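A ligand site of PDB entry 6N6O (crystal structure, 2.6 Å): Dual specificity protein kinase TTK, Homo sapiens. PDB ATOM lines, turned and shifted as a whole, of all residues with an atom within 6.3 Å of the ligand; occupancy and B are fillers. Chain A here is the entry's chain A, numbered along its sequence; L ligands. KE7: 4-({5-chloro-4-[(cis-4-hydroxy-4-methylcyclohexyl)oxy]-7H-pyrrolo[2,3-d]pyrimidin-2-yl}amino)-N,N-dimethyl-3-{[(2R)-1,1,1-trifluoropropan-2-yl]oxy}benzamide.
N3 of the ligand lies within hydrogen-bond range of N of Gly 93 (3.0 Å). O of Glu 91 is in hydrogen-bond range of N2 of the ligand, 2.8 Å away. N4 of the ligand lies within hydrogen-bond range of O of Gly 93.
The backbone NH of Ile 19 is in hydrogen-bond range of the backbone carbonyl oxygen of Val 27 (2.8 Å). The backbone carbonyl oxygen of Ala 39 is in hydrogen-bond range of the backbone NH of Met 90, at 2.7 Å. N of Asn 94 sits at hydrogen-bond distance from O of Ile 143 (2.7 Å). The side-chain hydroxyl (OG) of Ser 99 sits at hydrogen-bond distance from the side-chain carboxylate (OD1) of Asp 96, 2.6 Å away. O of Ile 95 sits at hydrogen-bond distance from N of Ile 143, at 2.8 Å. The backbone NH (N) of Gln 29 lies within hydrogen-bond range of the backbone carbonyl oxygen (O) of Lys 17, 2.8 Å away.
NE2 of Gln 29 lies close to F2 of the ligand (2.8 Å). The backbone carbonyl oxygen of Asn 94 lies close to an oxygen (O4) of the ligand (3.4 Å). Lys 17 touches the ligand (NZ to F3, 3.997 Å). CD1 of Ile 19 touches F2 of the ligand, at 3.4 Å. Val 27 touches the ligand. CB of Ala 39 touches N2 of the ligand (3.3 Å). CE of Met 90 touches CL1 of the ligand (3.6 Å). CA of Cys 92 touches N3 of the ligand, 3.9 Å away. CG1 of Ile 95 touches O3 of the ligand, at 3.6 Å. OD1 of Asp 96 touches C16 of the ligand, 3.5 Å away. OG of Ser 99 touches C21 of the ligand, at 3.5 Å. CD2 of Leu 142 touches C5 of the ligand, at 3.3 Å. Hydrophobic or aromatic side chains that line the ligand: Ile 19, Val 27, Ala 39, Met 90, Ile 95 and Leu 142. 14 residues have an atom within 4 Å of the ligand: Lys 17, Ile 19, Val 27, Gln 29, Ala 39, Met 90, Glu 91, Cys 92, Gly 93, Asn 94, Ile 95, Asp 96, Ser 99 and Leu 142.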
ATOM      1  N   LYS A  17      10.618 -12.295  34.492  1.00  0.00           N
ATOM      2  CA  LYS A  17      11.205 -10.954  34.416  1.00  0.00           C
ATOM      3  C   LYS A  17      11.916 -10.708  33.060  1.00  0.00           C
ATOM      4  O   LYS A  17      12.043 -11.616  32.249  1.00  0.00           O
ATOM      5  CB  LYS A  17      12.191 -10.769  35.563  1.00  0.00           C
ATOM      6  CG  LYS A  17      13.333 -11.796  35.608  1.00  0.00           C
ATOM      7  CD  LYS A  17      14.476 -11.329  36.517  1.00  0.00           C
ATOM      8  CE  LYS A  17      15.282 -10.235  35.843  1.00  0.00           C
ATOM      9  NZ  LYS A  17      16.378  -9.691  36.685  1.00  0.00           N
ATOM     10  N   GLN A  18      12.356  -9.462  32.827  1.00  0.00           N
ATOM     11  CA  GLN A  18      13.099  -9.047  31.659  1.00  0.00           C
ATOM     12  C   GLN A  18      14.565  -9.059  31.973  1.00  0.00           C
ATOM     13  O   GLN A  18      14.883  -8.748  33.081  1.00  0.00           O
ATOM     14  CB  GLN A  18      12.718  -7.645  31.254  1.00  0.00           C
ATOM     15  CG  GLN A  18      13.299  -7.212  29.895  1.00  0.00           C
ATOM     16  CD  GLN A  18      12.808  -5.836  29.432  1.00  0.00           C
ATOM     17  OE1 GLN A  18      13.564  -5.062  28.874  1.00  0.00           O
ATOM     18  NE2 GLN A  18      11.557  -5.552  29.665  1.00  0.00           N
ATOM     19  N   ILE A  19      15.428  -9.397  31.008  1.00  0.00           N
ATOM     20  CA  ILE A  19      16.899  -9.485  31.215  1.00  0.00           C
ATOM     21  C   ILE A  19      17.554  -8.330  30.498  1.00  0.00           C
ATOM     22  O   ILE A  19      17.525  -8.238  29.260  1.00  0.00           O
ATOM     23  CB  ILE A  19      17.464 -10.803  30.690  1.00  0.00           C
ATOM     24  CG1 ILE A  19      16.898 -11.982  31.495  1.00  0.00           C
ATOM     25  CG2 ILE A  19      18.974 -10.820  30.755  1.00  0.00           C
ATOM     26  CD1 ILE A  19      17.081 -13.366  30.862  1.00  0.00           C
ATOM     27  N   GLY A  20      18.150  -7.417  31.256  1.00  0.00           N
ATOM     28  CA  GLY A  20      18.561  -6.122  30.693  1.00  0.00           C
ATOM     29  C   GLY A  20      17.397  -5.202  30.305  1.00  0.00           C
ATOM     30  O   GLY A  20      16.321  -5.228  30.939  1.00  0.00           O
ATOM     31  N   SER A  21      17.639  -4.373  29.270  1.00  0.00           N
ATOM     32  CA  SER A  21      16.615  -3.468  28.676  1.00  0.00           C
ATOM     33  C   SER A  21      16.412  -3.714  27.161  1.00  0.00           C
ATOM     34  O   SER A  21      15.767  -4.692  26.777  1.00  0.00           O
ATOM     35  CB  SER A  21      16.939  -1.989  28.976  1.00  0.00           C
ATOM     36  OG  SER A  21      16.649  -1.697  30.313  1.00  0.00           O
ATOM     37  N   VAL A  27      14.775  -9.437  25.855  1.00  0.00           N
ATOM     38  CA  VAL A  27      14.949 -10.819  26.333  1.00  0.00           C
ATOM     39  C   VAL A  27      14.298 -10.965  27.695  1.00  0.00           C
ATOM     40  O   VAL A  27      14.403 -10.076  28.539  1.00  0.00           O
ATOM     41  CB  VAL A  27      16.433 -11.185  26.442  1.00  0.00           C
ATOM     42  CG1 VAL A  27      16.594 -12.672  26.754  1.00  0.00           C
ATOM     43  CG2 VAL A  27      17.137 -10.862  25.141  1.00  0.00           C
ATOM     44  N   PHE A  28      13.639 -12.095  27.892  1.00  0.00           N
ATOM     45  CA  PHE A  28      12.847 -12.369  29.086  1.00  0.00           C
ATOM     46  C   PHE A  28      13.239 -13.715  29.692  1.00  0.00           C
ATOM     47  O   PHE A  28      13.409 -14.689  28.963  1.00  0.00           O
ATOM     48  CB  PHE A  28      11.336 -12.490  28.756  1.00  0.00           C
ATOM     49  CG  PHE A  28      10.717 -11.227  28.267  1.00  0.00           C
ATOM     50  CD1 PHE A  28      10.594 -10.124  29.128  1.00  0.00           C
ATOM     51  CD2 PHE A  28      10.217 -11.120  26.980  1.00  0.00           C
ATOM     52  CE1 PHE A  28       9.995  -8.938  28.686  1.00  0.00           C
ATOM     53  CE2 PHE A  28       9.619  -9.948  26.536  1.00  0.00           C
ATOM     54  CZ  PHE A  28       9.506  -8.844  27.398  1.00  0.00           C
ATOM     55  N   GLN A  29      13.261 -13.802  31.024  1.00  0.00           N
ATOM     56  CA  GLN A  29      13.297 -15.091  31.715  1.00  0.00           C
ATOM     57  C   GLN A  29      11.871 -15.611  31.879  1.00  0.00           C
ATOM     58  O   GLN A  29      10.988 -14.849  32.197  1.00  0.00           O
ATOM     59  CB  GLN A  29      13.988 -14.936  33.050  1.00  0.00           C
ATOM     60  CG  GLN A  29      14.487 -16.249  33.671  1.00  0.00           C
ATOM     61  CD  GLN A  29      14.964 -16.065  35.108  1.00  0.00           C
ATOM     62  OE1 GLN A  29      14.241 -15.458  35.939  1.00  0.00           O
ATOM     63  NE2 GLN A  29      16.217 -16.468  35.399  1.00  0.00           N
ATOM     64  N   ALA A  39      15.257 -18.630  28.381  1.00  0.00           N
ATOM     65  CA  ALA A  39      15.298 -17.230  27.954  1.00  0.00           C
ATOM     66  C   ALA A  39      14.594 -17.117  26.600  1.00  0.00           C
ATOM     67  O   ALA A  39      14.830 -17.900  25.676  1.00  0.00           O
ATOM     68  CB  ALA A  39      16.711 -16.708  27.861  1.00  0.00           C
ATOM     69  N   ILE A  40      13.681 -16.163  26.511  1.00  0.00           N
ATOM     70  CA  ILE A  40      12.936 -15.975  25.295  1.00  0.00           C
ATOM     71  C   ILE A  40      13.286 -14.635  24.760  1.00  0.00           C
ATOM     72  O   ILE A  40      13.077 -13.618  25.461  1.00  0.00           O
ATOM     73  CB  ILE A  40      11.423 -16.087  25.497  1.00  0.00           C
ATOM     74  CG1 ILE A  40      11.090 -17.560  25.654  1.00  0.00           C
ATOM     75  CG2 ILE A  40      10.695 -15.490  24.305  1.00  0.00           C
ATOM     76  CD1 ILE A  40       9.626 -17.891  25.635  1.00  0.00           C
ATOM     77  N   LYS A  41      13.823 -14.627  23.545  1.00  0.00           N
ATOM     78  CA  LYS A  41      14.108 -13.385  22.852  1.00  0.00           C
ATOM     79  C   LYS A  41      12.892 -12.976  22.052  1.00  0.00           C
ATOM     80  O   LYS A  41      12.367 -13.801  21.248  1.00  0.00           O
ATOM     81  CB  LYS A  41      15.276 -13.544  21.908  1.00  0.00           C
ATOM     82  CG  LYS A  41      15.821 -12.234  21.442  1.00  0.00           C
ATOM     83  CD  LYS A  41      17.104 -12.453  20.695  1.00  0.00           C
ATOM     84  CE  LYS A  41      17.721 -11.091  20.373  1.00  0.00           C
ATOM     85  NZ  LYS A  41      18.870 -11.128  19.412  1.00  0.00           N
ATOM     86  N   ILE A  74      25.002 -21.401  22.351  1.00  0.00           N
ATOM     87  CA  ILE A  74      23.734 -21.393  23.078  1.00  0.00           C
ATOM     88  C   ILE A  74      22.702 -22.223  22.318  1.00  0.00           C
ATOM     89  O   ILE A  74      22.622 -22.121  21.073  1.00  0.00           O
ATOM     90  CB  ILE A  74      23.234 -19.910  23.250  1.00  0.00           C
ATOM     91  CG1 ILE A  74      22.389 -19.746  24.506  1.00  0.00           C
ATOM     92  CG2 ILE A  74      22.461 -19.438  22.036  1.00  0.00           C
ATOM     93  CD1 ILE A  74      23.219 -19.743  25.770  1.00  0.00           C
ATOM     94  N   MET A  90      15.404 -20.027  24.078  1.00  0.00           N
ATOM     95  CA  MET A  90      16.822 -20.363  24.261  1.00  0.00           C
ATOM     96  C   MET A  90      17.083 -20.859  25.681  1.00  0.00           C
ATOM     97  O   MET A  90      16.255 -20.665  26.582  1.00  0.00           O
ATOM     98  CB  MET A  90      17.670 -19.130  23.974  1.00  0.00           C
ATOM     99  CG  MET A  90      17.398 -18.620  22.554  1.00  0.00           C
ATOM    100  SD  MET A  90      18.604 -17.456  21.889  1.00  0.00           S
ATOM    101  CE  MET A  90      17.704 -15.998  22.271  1.00  0.00           C
ATOM    102  N   GLU A  91      18.220 -21.518  25.901  1.00  0.00           N
ATOM    103  CA  GLU A  91      18.618 -21.826  27.245  1.00  0.00           C
ATOM    104  C   GLU A  91      19.016 -20.538  27.937  1.00  0.00           C
ATOM    105  O   GLU A  91      19.490 -19.593  27.264  1.00  0.00           O
ATOM    106  CB  GLU A  91      19.726 -22.853  27.307  1.00  0.00           C
ATOM    107  CG  GLU A  91      21.135 -22.365  27.200  1.00  0.00           C
ATOM    108  CD  GLU A  91      22.065 -23.494  26.817  1.00  0.00           C
ATOM    109  OE1 GLU A  91      22.228 -24.380  27.665  1.00  0.00           O
ATOM    110  OE2 GLU A  91      22.626 -23.491  25.698  1.00  0.00           O
ATOM    111  N   CYS A  92      18.773 -20.504  29.257  1.00  0.00           N
ATOM    112  CA  CYS A  92      19.064 -19.330  30.042  1.00  0.00           C
ATOM    113  C   CYS A  92      20.474 -19.478  30.577  1.00  0.00           C
ATOM    114  O   CYS A  92      20.798 -20.505  31.164  1.00  0.00           O
ATOM    115  CB  CYS A  92      18.028 -19.131  31.202  1.00  0.00           C
ATOM    116  SG  CYS A  92      18.000 -17.425  31.880  1.00  0.00           S
ATOM    117  N   GLY A  93      21.314 -18.464  30.344  1.00  0.00           N
ATOM    118  CA  GLY A  93      22.601 -18.363  31.036  1.00  0.00           C
ATOM    119  C   GLY A  93      22.422 -17.733  32.421  1.00  0.00           C
ATOM    120  O   GLY A  93      21.409 -17.123  32.692  1.00  0.00           O
ATOM    121  N   ASN A  94      23.421 -17.889  33.276  1.00  0.00           N
ATOM    122  CA  ASN A  94      23.448 -17.274  34.596  1.00  0.00           C
ATOM    123  C   ASN A  94      23.597 -15.803  34.446  1.00  0.00           C
ATOM    124  O   ASN A  94      22.913 -15.013  35.069  1.00  0.00           O
ATOM    125  CB  ASN A  94      24.687 -17.725  35.407  1.00  0.00           C
ATOM    126  CG  ASN A  94      24.644 -19.181  35.823  1.00  0.00           C
ATOM    127  OD1 ASN A  94      24.226 -20.083  35.088  1.00  0.00           O
ATOM    128  ND2 ASN A  94      25.145 -19.431  37.012  1.00  0.00           N
ATOM    129  N   ILE A  95      24.570 -15.437  33.631  1.00  0.00           N
ATOM    130  CA  ILE A  95      25.042 -14.081  33.504  1.00  0.00           C
ATOM    131  C   ILE A  95      25.939 -14.021  32.238  1.00  0.00           C
ATOM    132  O   ILE A  95      26.372 -15.046  31.722  1.00  0.00           O
ATOM    133  CB  ILE A  95      25.826 -13.717  34.774  1.00  0.00           C
ATOM    134  CG1 ILE A  95      26.106 -12.231  34.858  1.00  0.00           C
ATOM    135  CG2 ILE A  95      27.110 -14.558  34.897  1.00  0.00           C
ATOM    136  CD1 ILE A  95      26.569 -11.818  36.254  1.00  0.00           C
ATOM    137  N   ASP A  96      26.153 -12.819  31.744  1.00  0.00           N
ATOM    138  CA  ASP A  96      27.039 -12.595  30.622  1.00  0.00           C
ATOM    139  C   ASP A  96      28.428 -12.321  31.164  1.00  0.00           C
ATOM    140  O   ASP A  96      28.595 -11.780  32.246  1.00  0.00           O
ATOM    141  CB  ASP A  96      26.578 -11.424  29.749  1.00  0.00           C
ATOM    142  CG  ASP A  96      26.601 -10.099  30.461  1.00  0.00           C
ATOM    143  OD1 ASP A  96      25.628  -9.797  31.199  1.00  0.00           O
ATOM    144  OD2 ASP A  96      27.601  -9.386  30.294  1.00  0.00           O
ATOM    145  N   SER A  99      29.339  -8.604  32.362  1.00  0.00           N
ATOM    146  CA  SER A  99      28.766  -8.299  33.671  1.00  0.00           C
ATOM    147  C   SER A  99      29.592  -8.929  34.785  1.00  0.00           C
ATOM    148  O   SER A  99      29.984  -8.253  35.737  1.00  0.00           O
ATOM    149  CB  SER A  99      27.318  -8.791  33.772  1.00  0.00           C
ATOM    150  OG  SER A  99      26.468  -8.016  32.949  1.00  0.00           O
ATOM    151  N   ALA A 139      30.640  -9.342  26.089  1.00  0.00           N
ATOM    152  CA  ALA A 139      29.155  -9.454  26.135  1.00  0.00           C
ATOM    153  C   ALA A 139      28.594 -10.467  25.169  1.00  0.00           C
ATOM    154  O   ALA A 139      27.435 -10.839  25.241  1.00  0.00           O
ATOM    155  CB  ALA A 139      28.474  -8.096  25.951  1.00  0.00           C
ATOM    156  N   LEU A 142      28.017 -15.927  27.251  1.00  0.00           N
ATOM    157  CA  LEU A 142      27.134 -16.170  28.363  1.00  0.00           C
ATOM    158  C   LEU A 142      27.647 -17.347  29.178  1.00  0.00           C
ATOM    159  O   LEU A 142      27.891 -18.439  28.614  1.00  0.00           O
ATOM    160  CB  LEU A 142      25.799 -16.559  27.816  1.00  0.00           C
ATOM    161  CG  LEU A 142      24.541 -16.083  28.512  1.00  0.00           C
ATOM    162  CD1 LEU A 142      24.408 -14.569  28.551  1.00  0.00           C
ATOM    163  CD2 LEU A 142      23.384 -16.692  27.764  1.00  0.00           C
ATOM    164  N   ILE A 143      27.743 -17.143  30.509  1.00  0.00           N
ATOM    165  CA  ILE A 143      28.114 -18.211  31.437  1.00  0.00           C
ATOM    166  C   ILE A 143      26.858 -19.018  31.722  1.00  0.00           C
ATOM    167  O   ILE A 143      25.877 -18.473  32.196  1.00  0.00           O
ATOM    168  CB  ILE A 143      28.735 -17.676  32.734  1.00  0.00           C
ATOM    169  CG1 ILE A 143      30.012 -16.902  32.403  1.00  0.00           C
ATOM    170  CG2 ILE A 143      29.151 -18.834  33.624  1.00  0.00           C
ATOM    171  CD1 ILE A 143      30.714 -16.180  33.535  1.00  0.00           C
ATOM    172  N   ILE A 151      26.697 -16.415  22.082  1.00  0.00           N
ATOM    173  CA  ILE A 151      25.275 -16.126  21.831  1.00  0.00           C
ATOM    174  C   ILE A 151      24.952 -15.465  20.503  1.00  0.00           C
ATOM    175  O   ILE A 151      23.838 -15.649  19.977  1.00  0.00           O
ATOM    176  CB  ILE A 151      24.614 -15.313  22.956  1.00  0.00           C
ATOM    177  CG1 ILE A 151      25.396 -14.062  23.279  1.00  0.00           C
ATOM    178  CG2 ILE A 151      24.507 -16.184  24.179  1.00  0.00           C
ATOM    179  CD1 ILE A 151      24.575 -13.043  24.031  1.00  0.00           C
HETATM  180  C1  KE7 L   1      20.768 -14.660  29.725  1.00  0.00           C
HETATM  181  C2  KE7 L   1      20.488 -13.485  27.740  1.00  0.00           C
HETATM  182  C3  KE7 L   1      20.995 -11.222  27.787  1.00  0.00           C
HETATM  183  C4  KE7 L   1      20.186 -14.682  27.094  1.00  0.00           C
HETATM  184  C5  KE7 L   1      20.184 -15.858  27.821  1.00  0.00           C
HETATM  185  C6  KE7 L   1      19.691 -16.357  25.765  1.00  0.00           C
HETATM  186  N1  KE7 L   1      20.763 -13.508  29.050  1.00  0.00           N
HETATM  187  N2  KE7 L   1      19.884 -16.845  26.987  1.00  0.00           N
HETATM  188  N3  KE7 L   1      20.475 -15.827  29.122  1.00  0.00           N
HETATM  189  O1  KE7 L   1      20.486 -12.330  27.052  1.00  0.00           O
HETATM  190  C7  KE7 L   1      19.863 -15.036  25.803  1.00  0.00           C
HETATM  191  C8  KE7 L   1      20.207 -10.031  27.259  1.00  0.00           C
HETATM  192  C9  KE7 L   1      20.778  -8.696  27.746  1.00  0.00           C
HETATM  193  C10 KE7 L   1      22.252  -8.543  27.393  1.00  0.00           C
HETATM  194  C11 KE7 L   1      23.026  -9.761  27.900  1.00  0.00           C
HETATM  195  C12 KE7 L   1      22.450 -11.068  27.366  1.00  0.00           C
HETATM  196  C13 KE7 L   1      22.799  -7.268  28.055  1.00  0.00           C
HETATM  197  C14 KE7 L   1      21.452 -13.592  31.708  1.00  0.00           C
HETATM  198  C15 KE7 L   1      22.344 -12.682  31.174  1.00  0.00           C
HETATM  199  O2  KE7 L   1      22.399  -8.480  25.981  1.00  0.00           O
HETATM  200 CL1  KE7 L   1      19.701 -13.974  24.441  1.00  0.00          CL
HETATM  201  N4  KE7 L   1      21.041 -14.661  31.031  1.00  0.00           N
HETATM  202  C16 KE7 L   1      22.747 -11.586  31.941  1.00  0.00           C
HETATM  203  C17 KE7 L   1      22.239 -11.385  33.228  1.00  0.00           C
HETATM  204  C20 KE7 L   1      22.679 -10.181  34.078  1.00  0.00           C
HETATM  205  O3  KE7 L   1      23.003 -10.356  35.246  1.00  0.00           O
HETATM  206  N5  KE7 L   1      22.727  -8.985  33.485  1.00  0.00           N
HETATM  207  C22 KE7 L   1      22.346  -8.836  32.072  1.00  0.00           C
HETATM  208  C21 KE7 L   1      23.184  -7.824  34.258  1.00  0.00           C
HETATM  209  C18 KE7 L   1      21.340 -12.309  33.758  1.00  0.00           C
HETATM  210  C19 KE7 L   1      20.956 -13.404  32.994  1.00  0.00           C
HETATM  211  O4  KE7 L   1      20.061 -14.329  33.438  1.00  0.00           O
HETATM  212  C23 KE7 L   1      19.703 -14.362  34.815  1.00  0.00           C
HETATM  213  C24 KE7 L   1      19.527 -15.856  35.138  1.00  0.00           C
HETATM  214  C25 KE7 L   1      18.342 -13.686  34.941  1.00  0.00           C
HETATM  215  F2  KE7 L   1      17.460 -14.286  34.129  1.00  0.00           F
HETATM  216  F3  KE7 L   1      18.467 -12.399  34.616  1.00  0.00           F
HETATM  217  F1  KE7 L   1      17.932 -13.798  36.187  1.00  0.00           F
